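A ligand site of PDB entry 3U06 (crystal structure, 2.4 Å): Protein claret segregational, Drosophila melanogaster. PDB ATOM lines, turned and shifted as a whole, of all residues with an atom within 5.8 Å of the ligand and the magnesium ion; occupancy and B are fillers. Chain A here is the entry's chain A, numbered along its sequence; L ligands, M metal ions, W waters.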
ATOM      1  N   ARG A  66       6.482 -13.493  25.657  1.00  0.00           N
ATOM      2  CA  ARG A  66       6.612 -14.606  24.705  1.00  0.00           C
ATOM      3  C   ARG A  66       5.963 -15.881  25.220  1.00  0.00           C
ATOM      4  O   ARG A  66       6.475 -16.528  26.126  1.00  0.00           O
ATOM      5  CB  ARG A  66       8.073 -14.877  24.356  1.00  0.00           C
ATOM      6  CG  ARG A  66       8.200 -15.913  23.239  1.00  0.00           C
ATOM      7  CD  ARG A  66       9.640 -16.258  22.898  1.00  0.00           C
ATOM      8  NE  ARG A  66       9.710 -16.958  21.623  1.00  0.00           N
ATOM      9  CZ  ARG A  66      10.796 -17.543  21.138  1.00  0.00           C
ATOM     10  NH1 ARG A  66      11.932 -17.516  21.820  1.00  0.00           N
ATOM     11  NH2 ARG A  66      10.753 -18.162  19.962  1.00  0.00           N
ATOM     12  N   ILE A  67       4.834 -16.232  24.620  1.00  0.00           N
ATOM     13  CA  ILE A  67       4.157 -17.485  24.925  1.00  0.00           C
ATOM     14  C   ILE A  67       4.749 -18.595  24.084  1.00  0.00           C
ATOM     15  O   ILE A  67       4.731 -18.516  22.850  1.00  0.00           O
ATOM     16  CB  ILE A  67       2.642 -17.406  24.606  1.00  0.00           C
ATOM     17  CG1 ILE A  67       2.045 -16.100  25.149  1.00  0.00           C
ATOM     18  CG2 ILE A  67       1.917 -18.616  25.167  1.00  0.00           C
ATOM     19  CD1 ILE A  67       2.382 -15.835  26.599  1.00  0.00           C
ATOM     20  N   ARG A  68       5.279 -19.635  24.728  1.00  0.00           N
ATOM     21  CA  ARG A  68       5.871 -20.735  23.968  1.00  0.00           C
ATOM     22  C   ARG A  68       4.823 -21.783  23.631  1.00  0.00           C
ATOM     23  O   ARG A  68       3.835 -21.943  24.343  1.00  0.00           O
ATOM     24  CB  ARG A  68       7.032 -21.384  24.735  1.00  0.00           C
ATOM     25  CG  ARG A  68       6.634 -22.295  25.887  1.00  0.00           C
ATOM     26  CD  ARG A  68       7.806 -23.186  26.263  1.00  0.00           C
ATOM     27  NE  ARG A  68       7.556 -24.033  27.429  1.00  0.00           N
ATOM     28  CZ  ARG A  68       6.985 -25.226  27.381  1.00  0.00           C
ATOM     29  NH1 ARG A  68       6.576 -25.742  26.238  1.00  0.00           N
ATOM     30  NH2 ARG A  68       6.814 -25.919  28.504  1.00  0.00           N
ATOM     31  N   PRO A  69       5.048 -22.504  22.512  1.00  0.00           N
ATOM     32  CA  PRO A  69       4.196 -23.631  22.125  1.00  0.00           C
ATOM     33  C   PRO A  69       4.402 -24.846  23.033  1.00  0.00           C
ATOM     34  O   PRO A  69       5.487 -24.992  23.589  1.00  0.00           O
ATOM     35  CB  PRO A  69       4.674 -23.969  20.709  1.00  0.00           C
ATOM     36  CG  PRO A  69       6.077 -23.461  20.661  1.00  0.00           C
ATOM     37  CD  PRO A  69       6.087 -22.233  21.510  1.00  0.00           C
ATOM     38  N   LEU A  71       5.232 -28.761  23.615  1.00  0.00           N
ATOM     39  CA  LEU A  71       6.001 -29.763  22.900  1.00  0.00           C
ATOM     40  C   LEU A  71       5.123 -30.979  22.651  1.00  0.00           C
ATOM     41  O   LEU A  71       4.089 -31.136  23.287  1.00  0.00           O
ATOM     42  CB  LEU A  71       7.247 -30.169  23.700  1.00  0.00           C
ATOM     43  CG  LEU A  71       8.303 -29.084  23.925  1.00  0.00           C
ATOM     44  CD1 LEU A  71       9.448 -29.642  24.737  1.00  0.00           C
ATOM     45  CD2 LEU A  71       8.806 -28.519  22.605  1.00  0.00           C
ATOM     46  N   PRO A 116       3.168 -18.417  20.153  1.00  0.00           N
ATOM     47  CA  PRO A 116       3.848 -19.701  19.909  1.00  0.00           C
ATOM     48  C   PRO A 116       4.460 -19.862  18.512  1.00  0.00           C
ATOM     49  O   PRO A 116       5.417 -20.635  18.366  1.00  0.00           O
ATOM     50  CB  PRO A 116       2.732 -20.729  20.128  1.00  0.00           C
ATOM     51  CG  PRO A 116       1.832 -20.079  21.113  1.00  0.00           C
ATOM     52  CD  PRO A 116       1.827 -18.630  20.726  1.00  0.00           C
ATOM     53  N   SER A 118       5.830 -17.308  16.878  1.00  0.00           N
ATOM     54  CA  SER A 118       6.917 -16.327  16.771  1.00  0.00           C
ATOM     55  C   SER A 118       8.275 -17.015  16.737  1.00  0.00           C
ATOM     56  O   SER A 118       8.622 -17.777  17.634  1.00  0.00           O
ATOM     57  CB  SER A 118       6.859 -15.349  17.941  1.00  0.00           C
ATOM     58  OG  SER A 118       5.660 -14.591  17.917  1.00  0.00           O
ATOM     59  N   GLN A 120      12.588 -17.450  16.350  1.00  0.00           N
ATOM     60  CA  GLN A 120      13.768 -16.936  17.041  1.00  0.00           C
ATOM     61  C   GLN A 120      14.202 -15.590  16.464  1.00  0.00           C
ATOM     62  O   GLN A 120      14.567 -14.676  17.199  1.00  0.00           O
ATOM     63  CB  GLN A 120      14.927 -17.927  16.919  1.00  0.00           C
ATOM     64  CG  GLN A 120      14.723 -19.241  17.675  1.00  0.00           C
ATOM     65  CD  GLN A 120      14.712 -19.062  19.184  1.00  0.00           C
ATOM     66  OE1 GLN A 120      14.001 -18.218  19.714  1.00  0.00           O
ATOM     67  NE2 GLN A 120      15.498 -19.883  19.878  1.00  0.00           N
ATOM     68  N   GLY A 146      10.825 -15.345  33.797  1.00  0.00           N
ATOM     69  CA  GLY A 146       9.694 -16.258  33.819  1.00  0.00           C
ATOM     70  C   GLY A 146       9.928 -17.503  34.633  1.00  0.00           C
ATOM     71  O   GLY A 146      11.036 -17.737  35.125  1.00  0.00           O
ATOM     72  N   GLN A 147       8.888 -18.323  34.772  1.00  0.00           N
ATOM     73  CA  GLN A 147       8.971 -19.535  35.568  1.00  0.00           C
ATOM     74  C   GLN A 147       9.661 -20.647  34.794  1.00  0.00           C
ATOM     75  O   GLN A 147       9.568 -20.721  33.572  1.00  0.00           O
ATOM     76  CB  GLN A 147       7.574 -19.989  36.010  1.00  0.00           C
ATOM     77  CG  GLN A 147       6.985 -21.118  35.184  1.00  0.00           C
ATOM     78  CD  GLN A 147       5.585 -21.519  35.635  1.00  0.00           C
ATOM     79  OE1 GLN A 147       4.589 -21.094  35.054  1.00  0.00           O
ATOM     80  NE2 GLN A 147       5.510 -22.332  36.676  1.00  0.00           N
ATOM     81  N   THR A 148      10.361 -21.516  35.528  1.00  0.00           N
ATOM     82  CA  THR A 148      11.022 -22.675  34.933  1.00  0.00           C
ATOM     83  C   THR A 148      10.076 -23.402  33.981  1.00  0.00           C
ATOM     84  O   THR A 148       8.937 -23.722  34.334  1.00  0.00           O
ATOM     85  CB  THR A 148      11.509 -23.671  36.003  1.00  0.00           C
ATOM     86  OG1 THR A 148      12.479 -23.053  36.842  1.00  0.00           O
ATOM     87  CG2 THR A 148      12.132 -24.900  35.353  1.00  0.00           C
ATOM     88  N   GLY A 149      10.568 -23.681  32.784  1.00  0.00           N
ATOM     89  CA  GLY A 149       9.785 -24.370  31.770  1.00  0.00           C
ATOM     90  C   GLY A 149       9.118 -23.408  30.790  1.00  0.00           C
ATOM     91  O   GLY A 149       8.543 -23.844  29.799  1.00  0.00           O
ATOM     92  N   SER A 150       9.189 -22.116  31.076  1.00  0.00           N
ATOM     93  CA  SER A 150       8.491 -21.126  30.266  1.00  0.00           C
ATOM     94  C   SER A 150       9.236 -20.805  28.961  1.00  0.00           C
ATOM     95  O   SER A 150       8.605 -20.470  27.959  1.00  0.00           O
ATOM     96  CB  SER A 150       8.248 -19.843  31.068  1.00  0.00           C
ATOM     97  OG  SER A 150       9.461 -19.313  31.575  1.00  0.00           O
ATOM     98  N   GLY A 151      10.566 -20.896  28.981  1.00  0.00           N
ATOM     99  CA  GLY A 151      11.345 -20.746  27.768  1.00  0.00           C
ATOM    100  C   GLY A 151      12.477 -19.736  27.801  1.00  0.00           C
ATOM    101  O   GLY A 151      12.862 -19.202  26.766  1.00  0.00           O
ATOM    102  N   LYS A 152      13.026 -19.487  28.987  1.00  0.00           N
ATOM    103  CA  LYS A 152      14.101 -18.513  29.130  1.00  0.00           C
ATOM    104  C   LYS A 152      15.364 -18.931  28.369  1.00  0.00           C
ATOM    105  O   LYS A 152      15.928 -18.159  27.600  1.00  0.00           O
ATOM    106  CB  LYS A 152      14.437 -18.314  30.612  1.00  0.00           C
ATOM    107  CG  LYS A 152      13.358 -17.588  31.397  1.00  0.00           C
ATOM    108  CD  LYS A 152      13.793 -17.336  32.834  1.00  0.00           C
ATOM    109  CE  LYS A 152      14.202 -18.614  33.553  1.00  0.00           C
ATOM    110  NZ  LYS A 152      13.070 -19.571  33.700  1.00  0.00           N
ATOM    111  N   THR A 153      15.801 -20.171  28.605  1.00  0.00           N
ATOM    112  CA  THR A 153      17.038 -20.657  28.009  1.00  0.00           C
ATOM    113  C   THR A 153      16.919 -20.816  26.501  1.00  0.00           C
ATOM    114  O   THR A 153      17.868 -20.564  25.768  1.00  0.00           O
ATOM    115  CB  THR A 153      17.462 -22.003  28.643  1.00  0.00           C
ATOM    116  OG1 THR A 153      17.704 -21.823  30.043  1.00  0.00           O
ATOM    117  CG2 THR A 153      18.720 -22.534  27.979  1.00  0.00           C
ATOM    118  N   TYR A 154      15.749 -21.240  26.035  1.00  0.00           N
ATOM    119  CA  TYR A 154      15.503 -21.411  24.612  1.00  0.00           C
ATOM    120  C   TYR A 154      15.569 -20.059  23.902  1.00  0.00           C
ATOM    121  O   TYR A 154      15.984 -19.958  22.748  1.00  0.00           O
ATOM    122  CB  TYR A 154      14.142 -22.050  24.373  1.00  0.00           C
ATOM    123  CG  TYR A 154      13.795 -22.210  22.905  1.00  0.00           C
ATOM    124  CD1 TYR A 154      14.166 -23.351  22.203  1.00  0.00           C
ATOM    125  CD2 TYR A 154      13.084 -21.226  22.234  1.00  0.00           C
ATOM    126  CE1 TYR A 154      13.851 -23.498  20.866  1.00  0.00           C
ATOM    127  CE2 TYR A 154      12.757 -21.367  20.892  1.00  0.00           C
ATOM    128  CZ  TYR A 154      13.136 -22.505  20.217  1.00  0.00           C
ATOM    129  OH  TYR A 154      12.813 -22.644  18.888  1.00  0.00           O
ATOM    130  N   THR A 155      15.131 -19.023  24.608  1.00  0.00           N
ATOM    131  CA  THR A 155      15.119 -17.673  24.063  1.00  0.00           C
ATOM    132  C   THR A 155      16.528 -17.077  24.025  1.00  0.00           C
ATOM    133  O   THR A 155      16.898 -16.419  23.054  1.00  0.00           O
ATOM    134  CB  THR A 155      14.194 -16.750  24.881  1.00  0.00           C
ATOM    135  OG1 THR A 155      12.860 -17.271  24.857  1.00  0.00           O
ATOM    136  CG2 THR A 155      14.187 -15.344  24.305  1.00  0.00           C
ATOM    137  N   VAL A 159      18.511 -23.675  20.534  1.00  0.00           N
ATOM    138  CA  VAL A 159      19.064 -24.958  20.143  1.00  0.00           C
ATOM    139  C   VAL A 159      19.676 -24.846  18.757  1.00  0.00           C
ATOM    140  O   VAL A 159      19.385 -23.910  18.022  1.00  0.00           O
ATOM    141  CB  VAL A 159      17.972 -26.061  20.155  1.00  0.00           C
ATOM    142  CG1 VAL A 159      17.364 -26.181  21.542  1.00  0.00           C
ATOM    143  CG2 VAL A 159      16.900 -25.763  19.122  1.00  0.00           C
ATOM    144  N   ARG A 251      27.307 -24.968  32.651  1.00  0.00           N
ATOM    145  CA  ARG A 251      26.054 -24.312  33.007  1.00  0.00           C
ATOM    146  C   ARG A 251      25.099 -25.296  33.677  1.00  0.00           C
ATOM    147  O   ARG A 251      24.798 -26.358  33.119  1.00  0.00           O
ATOM    148  CB  ARG A 251      25.419 -23.738  31.738  1.00  0.00           C
ATOM    149  CG  ARG A 251      24.026 -23.196  31.905  1.00  0.00           C
ATOM    150  CD  ARG A 251      24.009 -21.837  32.568  1.00  0.00           C
ATOM    151  NE  ARG A 251      22.643 -21.393  32.806  1.00  0.00           N
ATOM    152  CZ  ARG A 251      21.856 -20.886  31.868  1.00  0.00           C
ATOM    153  NH1 ARG A 251      22.289 -20.733  30.620  1.00  0.00           N
ATOM    154  NH2 ARG A 251      20.620 -20.518  32.172  1.00  0.00           N
ATOM    155  N   SER A 262      19.502 -25.479  39.267  1.00  0.00           N
ATOM    156  CA  SER A 262      19.410 -25.126  37.865  1.00  0.00           C
ATOM    157  C   SER A 262      18.325 -24.067  37.687  1.00  0.00           C
ATOM    158  O   SER A 262      18.522 -23.052  37.023  1.00  0.00           O
ATOM    159  CB  SER A 262      19.057 -26.360  37.025  1.00  0.00           C
ATOM    160  OG  SER A 262      18.904 -26.023  35.659  1.00  0.00           O
ATOM    161  N   ASP A 292      20.034 -14.840  31.347  1.00  0.00           N
ATOM    162  CA  ASP A 292      19.052 -15.896  31.520  1.00  0.00           C
ATOM    163  C   ASP A 292      18.727 -16.005  33.004  1.00  0.00           C
ATOM    164  O   ASP A 292      19.434 -16.675  33.750  1.00  0.00           O
ATOM    165  CB  ASP A 292      19.621 -17.215  31.017  1.00  0.00           C
ATOM    166  CG  ASP A 292      18.586 -18.314  30.944  1.00  0.00           C
ATOM    167  OD1 ASP A 292      17.535 -18.184  31.609  1.00  0.00           O
ATOM    168  OD2 ASP A 292      18.824 -19.316  30.243  1.00  0.00           O
ATOM    169  N   ASN A 358       8.947 -14.716  29.588  1.00  0.00           N
ATOM    170  CA  ASN A 358       8.573 -16.005  29.029  1.00  0.00           C
ATOM    171  C   ASN A 358       7.423 -16.627  29.796  1.00  0.00           C
ATOM    172  O   ASN A 358       7.385 -16.610  31.035  1.00  0.00           O
ATOM    173  CB  ASN A 358       9.778 -16.946  29.029  1.00  0.00           C
ATOM    174  CG  ASN A 358      10.876 -16.464  28.109  1.00  0.00           C
ATOM    175  OD1 ASN A 358      11.793 -15.768  28.537  1.00  0.00           O
ATOM    176  ND2 ASN A 358      10.792 -16.828  26.832  1.00  0.00           N
HETATM  177  P1  LIG L   1      13.323 -22.284  31.166  1.00  0.00           P
HETATM  178  O1  LIG L   1      13.233 -23.344  32.227  1.00  0.00           O
HETATM  179  O2  LIG L   1      12.458 -21.069  31.445  1.00  0.00           O
HETATM  180  O3  LIG L   1      14.743 -21.973  30.750  1.00  0.00           O
HETATM  181  P2  LIG L   1      13.520 -23.682  28.732  1.00  0.00           P
HETATM  182  O4  LIG L   1      14.241 -24.869  29.343  1.00  0.00           O
HETATM  183  O5  LIG L   1      14.313 -22.605  28.040  1.00  0.00           O
HETATM  184  O6  LIG L   1      12.642 -22.970  29.874  1.00  0.00           O
HETATM  185  O7  LIG L   1      12.408 -24.273  27.710  1.00  0.00           O
HETATM  186  C1  LIG L   1      11.561 -25.360  28.083  1.00  0.00           C
HETATM  187  C2  LIG L   1      11.530 -26.356  26.936  1.00  0.00           C
HETATM  188  O8  LIG L   1      10.599 -25.922  25.939  1.00  0.00           O
HETATM  189  C3  LIG L   1      12.890 -26.471  26.270  1.00  0.00           C
HETATM  190  O9  LIG L   1      13.268 -27.854  26.170  1.00  0.00           O
HETATM  191  C4  LIG L   1      12.741 -25.850  24.898  1.00  0.00           C
HETATM  192  O10 LIG L   1      13.353 -26.645  23.885  1.00  0.00           O
HETATM  193  C5  LIG L   1      11.236 -25.724  24.682  1.00  0.00           C
HETATM  194  N1  LIG L   1      10.873 -24.384  24.165  1.00  0.00           N
HETATM  195  C6  LIG L   1      10.853 -23.255  24.902  1.00  0.00           C
HETATM  196  N2  LIG L   1      10.449 -22.192  24.141  1.00  0.00           N
HETATM  197  C7  LIG L   1      10.200 -22.649  22.904  1.00  0.00           C
HETATM  198  C8  LIG L   1       9.752 -22.070  21.621  1.00  0.00           C
HETATM  199  N3  LIG L   1       9.476 -20.740  21.488  1.00  0.00           N
HETATM  200  N4  LIG L   1       9.616 -22.904  20.560  1.00  0.00           N
HETATM  201  C9  LIG L   1       9.889 -24.225  20.648  1.00  0.00           C
HETATM  202  N5  LIG L   1      10.299 -24.808  21.779  1.00  0.00           N
HETATM  203  C10 LIG L   1      10.478 -24.098  22.924  1.00  0.00           C
HETATM  204 MG    MG M   1      16.653 -22.541  31.753  1.00  0.00          MG
HETATM  205  O   HOH W   1       7.282 -18.282  20.821  1.00  0.00           O
HETATM  206  O   HOH W   2      13.496 -26.335  32.259  1.00  0.00           O
HETATM  207  O   HOH W   3      15.630 -23.224  33.405  1.00  0.00           O
HETATM  208  O   HOH W   4      16.761 -20.672  32.634  1.00  0.00           O
HETATM  209  O   HOH W   5      16.536 -24.425  30.899  1.00  0.00           O
HETATM  210  O   HOH W   6      10.285 -19.542  24.376  1.00  0.00           O
HETATM  211  O   HOH W   7      18.460 -23.043  32.667  1.00  0.00           O
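The magnesium ion is bound by water W3 (2.1 Å), water W4 (2.1 Å), water W5 (2.1 Å), water W7 (2.1 Å), the side-chain hydroxyl (OG1) of Thr 153 (2.1 Å) and an oxygen (O3) of the ligand (2.2 Å).
The backbone carbonyl oxygen (O) of Gly 149 is in hydrogen-bond range of the guanidinium group (NE) of Arg 68.
O of Gly 146 lies within hydrogen-bond range of NZ of Lys 152 (3.1 Å).
The backbone carbonyl oxygen (O) of Gly 151 is in hydrogen-bond range of the side-chain hydroxyl (OG1) of Thr 155 (2.7 Å).
The backbone carbonyl oxygen (O) of Gly 151 sits at hydrogen-bond distance from the side-chain amide nitrogen (ND2) of Asn 358.
NH2 of Arg 66 lies within hydrogen-bond range of O of Ser 118 (3.2 Å).
The side-chain amide oxygen (OE1) of Gln 120 is in hydrogen-bond range of the guanidinium group (NH1) of Arg 66 (3.0 Å).
O of Gln 147 is in hydrogen-bond range of OG of Ser 150 (2.4 Å).
OG of Ser 150 sits close to O of Asn 358, at 3.5 Å.
N3 of the ligand lies close to NH2 of Arg 66, 3.3 Å away.
CD of Arg 68 touches C6 of the ligand, 3.3 Å away.
Pro 69 touches the ligand.
Gln 147 touches the ligand.
Thr 148 touches the ligand.
11 residues have an atom within 4 Å of the ligand: Arg 66, Arg 68, Pro 69, Gln 147, Thr 148, Gly 149, Ser 150, Gly 151, Lys 152, Thr 153 and Tyr 154.
The nearest printed residue that does not touch the ligand is Leu 71 (4.1 Å).
N of Thr 153 lies within hydrogen-bond range of O5 of the ligand, at 2.9 Å.
N of Gly 149 sits at hydrogen-bond distance from O1 of the ligand (2.7 Å).
O2 of the ligand sits at hydrogen-bond distance from N of Lys 152 (3.0 Å).
O2 of the ligand lies within salt-bridge range of NZ of Lys 152.
The backbone NH (N) of Tyr 154 sits at hydrogen-bond distance from an oxygen (O5) of the ligand (2.8 Å).
The backbone NH (N) of Gly 151 lies within hydrogen-bond range of an oxygen (O6) of the ligand (3.1 Å).
An oxygen (O2) of the ligand lies within hydrogen-bond range of the backbone NH (N) of Ser 150 (3.5 Å).
The side-chain hydroxyl (OG) of Ser 150 lies within hydrogen-bond range of an oxygen (O2) of the ligand (3.5 Å).
Water W6 bridges N2 of the ligand and OG1 of Thr 155.
Water W1 lies within hydrogen-bond range of NE of Arg 66 (2.9 Å), O of Ile 67 (3.3 Å), N3 of the ligand (3.4 Å) and O of Ser 118 (3.5 Å).
Within 4 Å of the magnesium ion: Thr 153.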
